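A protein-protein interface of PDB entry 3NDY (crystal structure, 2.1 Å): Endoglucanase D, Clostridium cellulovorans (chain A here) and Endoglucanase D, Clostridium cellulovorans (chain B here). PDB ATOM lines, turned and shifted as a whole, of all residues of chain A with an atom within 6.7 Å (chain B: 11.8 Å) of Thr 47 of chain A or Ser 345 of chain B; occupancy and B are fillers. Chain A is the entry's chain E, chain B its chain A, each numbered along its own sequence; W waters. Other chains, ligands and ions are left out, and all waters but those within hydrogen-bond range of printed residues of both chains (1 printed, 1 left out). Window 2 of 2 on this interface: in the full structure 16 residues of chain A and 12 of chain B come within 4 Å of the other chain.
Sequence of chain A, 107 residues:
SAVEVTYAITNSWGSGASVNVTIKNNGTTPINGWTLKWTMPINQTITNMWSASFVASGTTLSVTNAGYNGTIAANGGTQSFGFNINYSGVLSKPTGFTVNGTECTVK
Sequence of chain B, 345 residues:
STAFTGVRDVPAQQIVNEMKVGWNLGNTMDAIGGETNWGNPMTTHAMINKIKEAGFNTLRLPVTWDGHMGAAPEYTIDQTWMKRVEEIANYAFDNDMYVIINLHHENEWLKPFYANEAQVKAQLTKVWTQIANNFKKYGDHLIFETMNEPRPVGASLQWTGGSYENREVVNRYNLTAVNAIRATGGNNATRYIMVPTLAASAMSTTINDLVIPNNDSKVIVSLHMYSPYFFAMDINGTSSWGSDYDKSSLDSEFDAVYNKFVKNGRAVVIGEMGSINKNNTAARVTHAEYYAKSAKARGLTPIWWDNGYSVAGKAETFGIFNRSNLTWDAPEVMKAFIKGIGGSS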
ATOM      1  N   TRP A  13     -22.682   3.364  28.279  1.00  0.00           N
ATOM      2  CA  TRP A  13     -21.780   2.235  28.487  1.00  0.00           C
ATOM      3  C   TRP A  13     -21.480   2.007  29.966  1.00  0.00           C
ATOM      4  O   TRP A  13     -20.350   1.686  30.338  1.00  0.00           O
ATOM      5  CB  TRP A  13     -20.474   2.445  27.715  1.00  0.00           C
ATOM      6  CG  TRP A  13     -19.874   3.808  27.909  1.00  0.00           C
ATOM      7  CD1 TRP A  13     -18.980   4.182  28.874  1.00  0.00           C
ATOM      8  CD2 TRP A  13     -20.129   4.981  27.121  1.00  0.00           C
ATOM      9  NE1 TRP A  13     -18.663   5.512  28.733  1.00  0.00           N
ATOM     10  CE2 TRP A  13     -19.352   6.027  27.665  1.00  0.00           C
ATOM     11  CE3 TRP A  13     -20.937   5.249  26.009  1.00  0.00           C
ATOM     12  CZ2 TRP A  13     -19.364   7.321  27.138  1.00  0.00           C
ATOM     13  CZ3 TRP A  13     -20.945   6.534  25.484  1.00  0.00           C
ATOM     14  CH2 TRP A  13     -20.164   7.555  26.052  1.00  0.00           C
ATOM     15  N   ALA A  17     -21.976   8.009  29.361  1.00  0.00           N
ATOM     16  CA  ALA A  17     -23.053   8.140  28.386  1.00  0.00           C
ATOM     17  C   ALA A  17     -22.797   9.320  27.462  1.00  0.00           C
ATOM     18  O   ALA A  17     -22.002  10.203  27.773  1.00  0.00           O
ATOM     19  CB  ALA A  17     -24.401   8.317  29.100  1.00  0.00           C
ATOM     20  N   THR A  45     -20.006  13.776  35.699  1.00  0.00           N
ATOM     21  CA  THR A  45     -19.002  14.731  35.256  1.00  0.00           C
ATOM     22  C   THR A  45     -19.004  14.787  33.734  1.00  0.00           C
ATOM     23  O   THR A  45     -18.972  13.746  33.072  1.00  0.00           O
ATOM     24  CB  THR A  45     -17.595  14.340  35.742  1.00  0.00           C
ATOM     25  OG1 THR A  45     -17.568  14.327  37.174  1.00  0.00           O
ATOM     26  CG2 THR A  45     -16.557  15.332  35.234  1.00  0.00           C
ATOM     27  N   ILE A  46     -19.050  15.999  33.184  1.00  0.00           N
ATOM     28  CA  ILE A  46     -18.957  16.181  31.738  1.00  0.00           C
ATOM     29  C   ILE A  46     -17.511  16.094  31.291  1.00  0.00           C
ATOM     30  O   ILE A  46     -16.675  16.885  31.721  1.00  0.00           O
ATOM     31  CB  ILE A  46     -19.542  17.536  31.278  1.00  0.00           C
ATOM     32  CG1 ILE A  46     -21.057  17.548  31.449  1.00  0.00           C
ATOM     33  CG2 ILE A  46     -19.205  17.789  29.815  1.00  0.00           C
ATOM     34  CD1 ILE A  46     -21.717  18.795  30.890  1.00  0.00           C
ATOM     35  N   THR A  47     -17.217  15.141  30.413  1.00  0.00           N
ATOM     36  CA  THR A  47     -15.848  14.935  29.966  1.00  0.00           C
ATOM     37  C   THR A  47     -15.511  15.773  28.741  1.00  0.00           C
ATOM     38  O   THR A  47     -14.389  16.277  28.604  1.00  0.00           O
ATOM     39  CB  THR A  47     -15.577  13.462  29.654  1.00  0.00           C
ATOM     40  OG1 THR A  47     -16.428  13.029  28.587  1.00  0.00           O
ATOM     41  CG2 THR A  47     -15.826  12.616  30.894  1.00  0.00           C
ATOM     42  N   ASN A  48     -16.474  15.901  27.837  1.00  0.00           N
ATOM     43  CA  ASN A  48     -16.316  16.822  26.726  1.00  0.00           C
ATOM     44  C   ASN A  48     -17.617  17.140  26.006  1.00  0.00           C
ATOM     45  O   ASN A  48     -18.607  16.414  26.130  1.00  0.00           O
ATOM     46  CB  ASN A  48     -15.227  16.366  25.757  1.00  0.00           C
ATOM     47  CG  ASN A  48     -15.561  15.076  25.084  1.00  0.00           C
ATOM     48  OD1 ASN A  48     -15.890  14.088  25.740  1.00  0.00           O
ATOM     49  ND2 ASN A  48     -15.477  15.064  23.759  1.00  0.00           N
ATOM     50  N   MET A  49     -17.601  18.245  25.268  1.00  0.00           N
ATOM     51  CA  MET A  49     -18.814  18.830  24.715  1.00  0.00           C
ATOM     52  C   MET A  49     -18.526  19.336  23.308  1.00  0.00           C
ATOM     53  O   MET A  49     -17.416  19.782  23.023  1.00  0.00           O
ATOM     54  CB  MET A  49     -19.277  19.981  25.618  1.00  0.00           C
ATOM     55  CG  MET A  49     -20.567  20.653  25.203  1.00  0.00           C
ATOM     56  SD  MET A  49     -21.061  21.964  26.352  1.00  0.00           S
ATOM     57  CE  MET A  49     -21.738  21.039  27.735  1.00  0.00           C
ATOM     58  N   PHE A  54     -18.824  25.020  28.126  1.00  0.00           N
ATOM     59  CA  PHE A  54     -19.453  25.044  29.434  1.00  0.00           C
ATOM     60  C   PHE A  54     -18.539  25.522  30.548  1.00  0.00           C
ATOM     61  O   PHE A  54     -17.315  25.575  30.404  1.00  0.00           O
ATOM     62  CB  PHE A  54     -20.057  23.671  29.783  1.00  0.00           C
ATOM     63  CG  PHE A  54     -19.035  22.603  30.078  1.00  0.00           C
ATOM     64  CD1 PHE A  54     -18.503  21.833  29.059  1.00  0.00           C
ATOM     65  CD2 PHE A  54     -18.625  22.355  31.384  1.00  0.00           C
ATOM     66  CE1 PHE A  54     -17.576  20.852  29.328  1.00  0.00           C
ATOM     67  CE2 PHE A  54     -17.697  21.370  31.666  1.00  0.00           C
ATOM     68  CZ  PHE A  54     -17.168  20.616  30.633  1.00  0.00           C
ATOM     69  N   PHE A  83     -22.776  16.219  24.511  1.00  0.00           N
ATOM     70  CA  PHE A  83     -21.615  15.994  25.369  1.00  0.00           C
ATOM     71  C   PHE A  83     -21.536  14.564  25.882  1.00  0.00           C
ATOM     72  O   PHE A  83     -22.526  13.821  25.851  1.00  0.00           O
ATOM     73  CB  PHE A  83     -21.600  16.962  26.559  1.00  0.00           C
ATOM     74  CG  PHE A  83     -22.857  16.945  27.391  1.00  0.00           C
ATOM     75  CD1 PHE A  83     -23.944  17.737  27.046  1.00  0.00           C
ATOM     76  CD2 PHE A  83     -22.937  16.166  28.540  1.00  0.00           C
ATOM     77  CE1 PHE A  83     -25.097  17.743  27.824  1.00  0.00           C
ATOM     78  CE2 PHE A  83     -24.083  16.159  29.319  1.00  0.00           C
ATOM     79  CZ  PHE A  83     -25.168  16.951  28.965  1.00  0.00           C
ATOM     80  N   ASN A  84     -20.349  14.194  26.359  1.00  0.00           N
ATOM     81  CA  ASN A  84     -20.140  12.931  27.060  1.00  0.00           C
ATOM     82  C   ASN A  84     -20.040  13.161  28.557  1.00  0.00           C
ATOM     83  O   ASN A  84     -19.492  14.172  29.003  1.00  0.00           O
ATOM     84  CB  ASN A  84     -18.868  12.244  26.568  1.00  0.00           C
ATOM     85  CG  ASN A  84     -18.983  11.754  25.141  1.00  0.00           C
ATOM     86  OD1 ASN A  84     -20.076  11.435  24.662  1.00  0.00           O
ATOM     87  ND2 ASN A  84     -17.854  11.694  24.451  1.00  0.00           N
ATOM     88  N   ILE A  85     -20.582  12.225  29.330  1.00  0.00           N
ATOM     89  CA  ILE A  85     -20.457  12.256  30.778  1.00  0.00           C
ATOM     90  C   ILE A  85     -19.813  10.973  31.295  1.00  0.00           C
ATOM     91  O   ILE A  85     -19.673   9.989  30.569  1.00  0.00           O
ATOM     92  CB  ILE A  85     -21.825  12.404  31.478  1.00  0.00           C
ATOM     93  CG1 ILE A  85     -22.750  11.248  31.093  1.00  0.00           C
ATOM     94  CG2 ILE A  85     -22.466  13.739  31.153  1.00  0.00           C
ATOM     95  CD1 ILE A  85     -24.097  11.318  31.742  1.00  0.00           C
ATOM     96  N   ASN A  86     -19.401  11.011  32.556  1.00  0.00           N
ATOM     97  CA  ASN A  86     -19.070   9.812  33.307  1.00  0.00           C
ATOM     98  C   ASN A  86     -20.024   9.793  34.478  1.00  0.00           C
ATOM     99  O   ASN A  86     -20.340  10.847  35.033  1.00  0.00           O
ATOM    100  CB  ASN A  86     -17.623   9.848  33.798  1.00  0.00           C
ATOM    101  CG  ASN A  86     -16.627   9.540  32.696  1.00  0.00           C
ATOM    102  OD1 ASN A  86     -16.932   8.814  31.749  1.00  0.00           O
ATOM    103  ND2 ASN A  86     -15.423  10.087  32.819  1.00  0.00           N
ATOM    104  N   ASN B  17     -13.863  30.584  17.300  1.00  0.00           N
ATOM    105  CA  ASN B  17     -14.135  29.693  18.430  1.00  0.00           C
ATOM    106  C   ASN B  17     -12.866  29.030  18.961  1.00  0.00           C
ATOM    107  O   ASN B  17     -12.657  28.964  20.168  1.00  0.00           O
ATOM    108  CB  ASN B  17     -15.143  28.608  18.046  1.00  0.00           C
ATOM    109  CG  ASN B  17     -16.545  29.149  17.880  1.00  0.00           C
ATOM    110  OD1 ASN B  17     -16.831  30.299  18.227  1.00  0.00           O
ATOM    111  ND2 ASN B  17     -17.433  28.320  17.347  1.00  0.00           N
ATOM    112  N   LYS B  20     -10.501  31.186  20.915  1.00  0.00           N
ATOM    113  CA  LYS B  20     -11.005  31.006  22.280  1.00  0.00           C
ATOM    114  C   LYS B  20     -10.901  32.227  23.198  1.00  0.00           C
ATOM    115  O   LYS B  20     -11.916  32.776  23.612  1.00  0.00           O
ATOM    116  CB  LYS B  20     -10.357  29.788  22.953  1.00  0.00           C
ATOM    117  CG  LYS B  20     -11.085  29.347  24.218  1.00  0.00           C
ATOM    118  CD  LYS B  20     -10.551  28.006  24.758  1.00  0.00           C
ATOM    119  CE  LYS B  20     -11.283  27.637  26.041  1.00  0.00           C
ATOM    120  NZ  LYS B  20     -10.691  26.485  26.760  1.00  0.00           N
ATOM    121  N   GLY B  55      -4.133  29.249  30.104  1.00  0.00           N
ATOM    122  CA  GLY B  55      -5.388  28.942  29.420  1.00  0.00           C
ATOM    123  C   GLY B  55      -5.696  29.782  28.181  1.00  0.00           C
ATOM    124  O   GLY B  55      -6.748  29.623  27.556  1.00  0.00           O
ATOM    125  N   ILE B 338     -10.122  33.764  32.475  1.00  0.00           N
ATOM    126  CA  ILE B 338     -10.057  32.423  31.894  1.00  0.00           C
ATOM    127  C   ILE B 338     -11.268  31.570  32.304  1.00  0.00           C
ATOM    128  O   ILE B 338     -11.855  30.866  31.472  1.00  0.00           O
ATOM    129  CB  ILE B 338      -8.749  31.694  32.306  1.00  0.00           C
ATOM    130  CG1 ILE B 338      -7.525  32.431  31.755  1.00  0.00           C
ATOM    131  CG2 ILE B 338      -8.761  30.249  31.842  1.00  0.00           C
ATOM    132  CD1 ILE B 338      -7.529  32.627  30.228  1.00  0.00           C
ATOM    133  N   LYS B 339     -11.641  31.644  33.581  1.00  0.00           N
ATOM    134  CA  LYS B 339     -12.782  30.887  34.099  1.00  0.00           C
ATOM    135  C   LYS B 339     -14.074  31.256  33.382  1.00  0.00           C
ATOM    136  O   LYS B 339     -14.891  30.389  33.078  1.00  0.00           O
ATOM    137  CB  LYS B 339     -12.948  31.129  35.604  1.00  0.00           C
ATOM    138  CG  LYS B 339     -14.110  30.378  36.243  1.00  0.00           C
ATOM    139  CD  LYS B 339     -14.191  30.696  37.740  1.00  0.00           C
ATOM    140  CE  LYS B 339     -15.175  29.787  38.477  1.00  0.00           C
ATOM    141  NZ  LYS B 339     -16.579  29.944  37.996  1.00  0.00           N
ATOM    142  N   GLY B 340     -14.259  32.547  33.116  1.00  0.00           N
ATOM    143  CA  GLY B 340     -15.463  33.013  32.449  1.00  0.00           C
ATOM    144  C   GLY B 340     -15.588  32.500  31.025  1.00  0.00           C
ATOM    145  O   GLY B 340     -16.695  32.352  30.512  1.00  0.00           O
ATOM    146  N   ILE B 341     -14.448  32.248  30.383  1.00  0.00           N
ATOM    147  CA  ILE B 341     -14.405  31.758  29.007  1.00  0.00           C
ATOM    148  C   ILE B 341     -14.956  30.330  28.873  1.00  0.00           C
ATOM    149  O   ILE B 341     -15.571  29.985  27.861  1.00  0.00           O
ATOM    150  CB  ILE B 341     -12.958  31.792  28.443  1.00  0.00           C
ATOM    151  CG1 ILE B 341     -12.486  33.236  28.255  1.00  0.00           C
ATOM    152  CG2 ILE B 341     -12.864  31.012  27.131  1.00  0.00           C
ATOM    153  CD1 ILE B 341     -13.264  34.028  27.199  1.00  0.00           C
ATOM    154  N   GLY B 342     -14.722  29.494  29.880  1.00  0.00           N
ATOM    155  CA  GLY B 342     -15.195  28.123  29.828  1.00  0.00           C
ATOM    156  C   GLY B 342     -14.369  27.283  28.869  1.00  0.00           C
ATOM    157  O   GLY B 342     -13.251  27.657  28.498  1.00  0.00           O
ATOM    158  N   GLY B 343     -14.918  26.142  28.463  1.00  0.00           N
ATOM    159  CA  GLY B 343     -14.216  25.238  27.572  1.00  0.00           C
ATOM    160  C   GLY B 343     -15.036  24.023  27.171  1.00  0.00           C
ATOM    161  O   GLY B 343     -16.175  23.846  27.607  1.00  0.00           O
ATOM    162  N   SER B 344     -14.449  23.169  26.342  1.00  0.00           N
ATOM    163  CA  SER B 344     -15.168  22.014  25.818  1.00  0.00           C
ATOM    164  C   SER B 344     -14.853  20.736  26.590  1.00  0.00           C
ATOM    165  O   SER B 344     -15.353  19.661  26.245  1.00  0.00           O
ATOM    166  CB  SER B 344     -14.847  21.830  24.333  1.00  0.00           C
ATOM    167  OG  SER B 344     -13.450  21.690  24.133  1.00  0.00           O
ATOM    168  N   SER B 345     -14.025  20.856  27.628  1.00  0.00           N
ATOM    169  CA  SER B 345     -13.598  19.706  28.427  1.00  0.00           C
ATOM    170  C   SER B 345     -13.661  20.037  29.909  1.00  0.00           C
ATOM    171  O   SER B 345     -13.370  21.165  30.312  1.00  0.00           O
ATOM    172  CB  SER B 345     -12.166  19.282  28.068  1.00  0.00           C
ATOM    173  OG  SER B 345     -12.062  18.866  26.711  1.00  0.00           O
HETATM  174  O   HOH W   1     -18.586  28.485  28.299  1.00  0.00           O
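The backbone NH of Met 49 of chain A lies within hydrogen-bond range of the backbone carbonyl oxygen of Ser 344 of chain B (2.8 Å). O of Gly 343 of chain B lies within hydrogen-bond range of N of Phe 54 of chain A, 2.9 Å away.
The backbone carbonyl oxygen of Gly 342 of chain B lies close to the side-chain amino group of Lys 20 of chain B (3.3 Å). The backbone NH of Thr 47 of chain A is in hydrogen-bond range of the backbone carbonyl oxygen of Asn 84 of chain A (2.8 Å). N of Asn 84 of chain A lies within hydrogen-bond range of O of Asn 48 of chain A. OD1 of Asn 48 of chain A is in hydrogen-bond range of OG1 of Thr 47 of chain A (3.1 Å).
Among the printed residues, merely in contact across the chains: Asn 48 of chain A with Ser 344 of chain B, Phe 54 of chain A with Gly 342 of chain B, Thr 47 of chain A with Ser 345 of chain B, Phe 54 of chain A with Ser 345 of chain B and Phe 54 of chain A with Ser 344 of chain B.
No residue of chain B comes within 4 Å of Thr 45 of chain A. No residue of chain B comes within 4 Å of Ile 46 of chain A. Of the printed residues of chain B, Thr 47 of chain A touches Ser 345. Of the printed residues of chain B, Asn 48 of chain A touches Ser 344 (3.0 Å). Met 49 of chain A touches just one residue of chain B: Ser 344 (2.8 Å). No residue of chain B comes within 4 Å of Asn 86 of chain A. Gly 55 of chain B touches none of the printed residues of chain A. Of the printed residues of chain A, Gly 342 of chain B touches Phe 54 (3.4 Å). Printed residues of chain A within 4 Å of Gly 343 of chain B: Phe 54. Printed residues of chain A within 4 Å of Ser 344 of chain B: Asn 48, Met 49 and Phe 54. The nearest printed residue of chain A that does not touch Gly 343 of chain B is Met 49 of chain A (5.3 Å).
Printed residues of chain B that touch a printed residue of chain A: Gly 342, Gly 343, Ser 344 and Ser 345. Along chain B the printed residues that touch a printed residue of chain A span positions 342 to 345. Of the 12 printed residues of chain A, 4 touch a printed residue of chain B. Among the printed residues, no Asp or Glu carboxylate lies within 4 Å of a Lys or Arg side-chain nitrogen of the other chain.
Water W1 bridges O of Ile 341 of chain B and N of Phe 54 of chain A.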
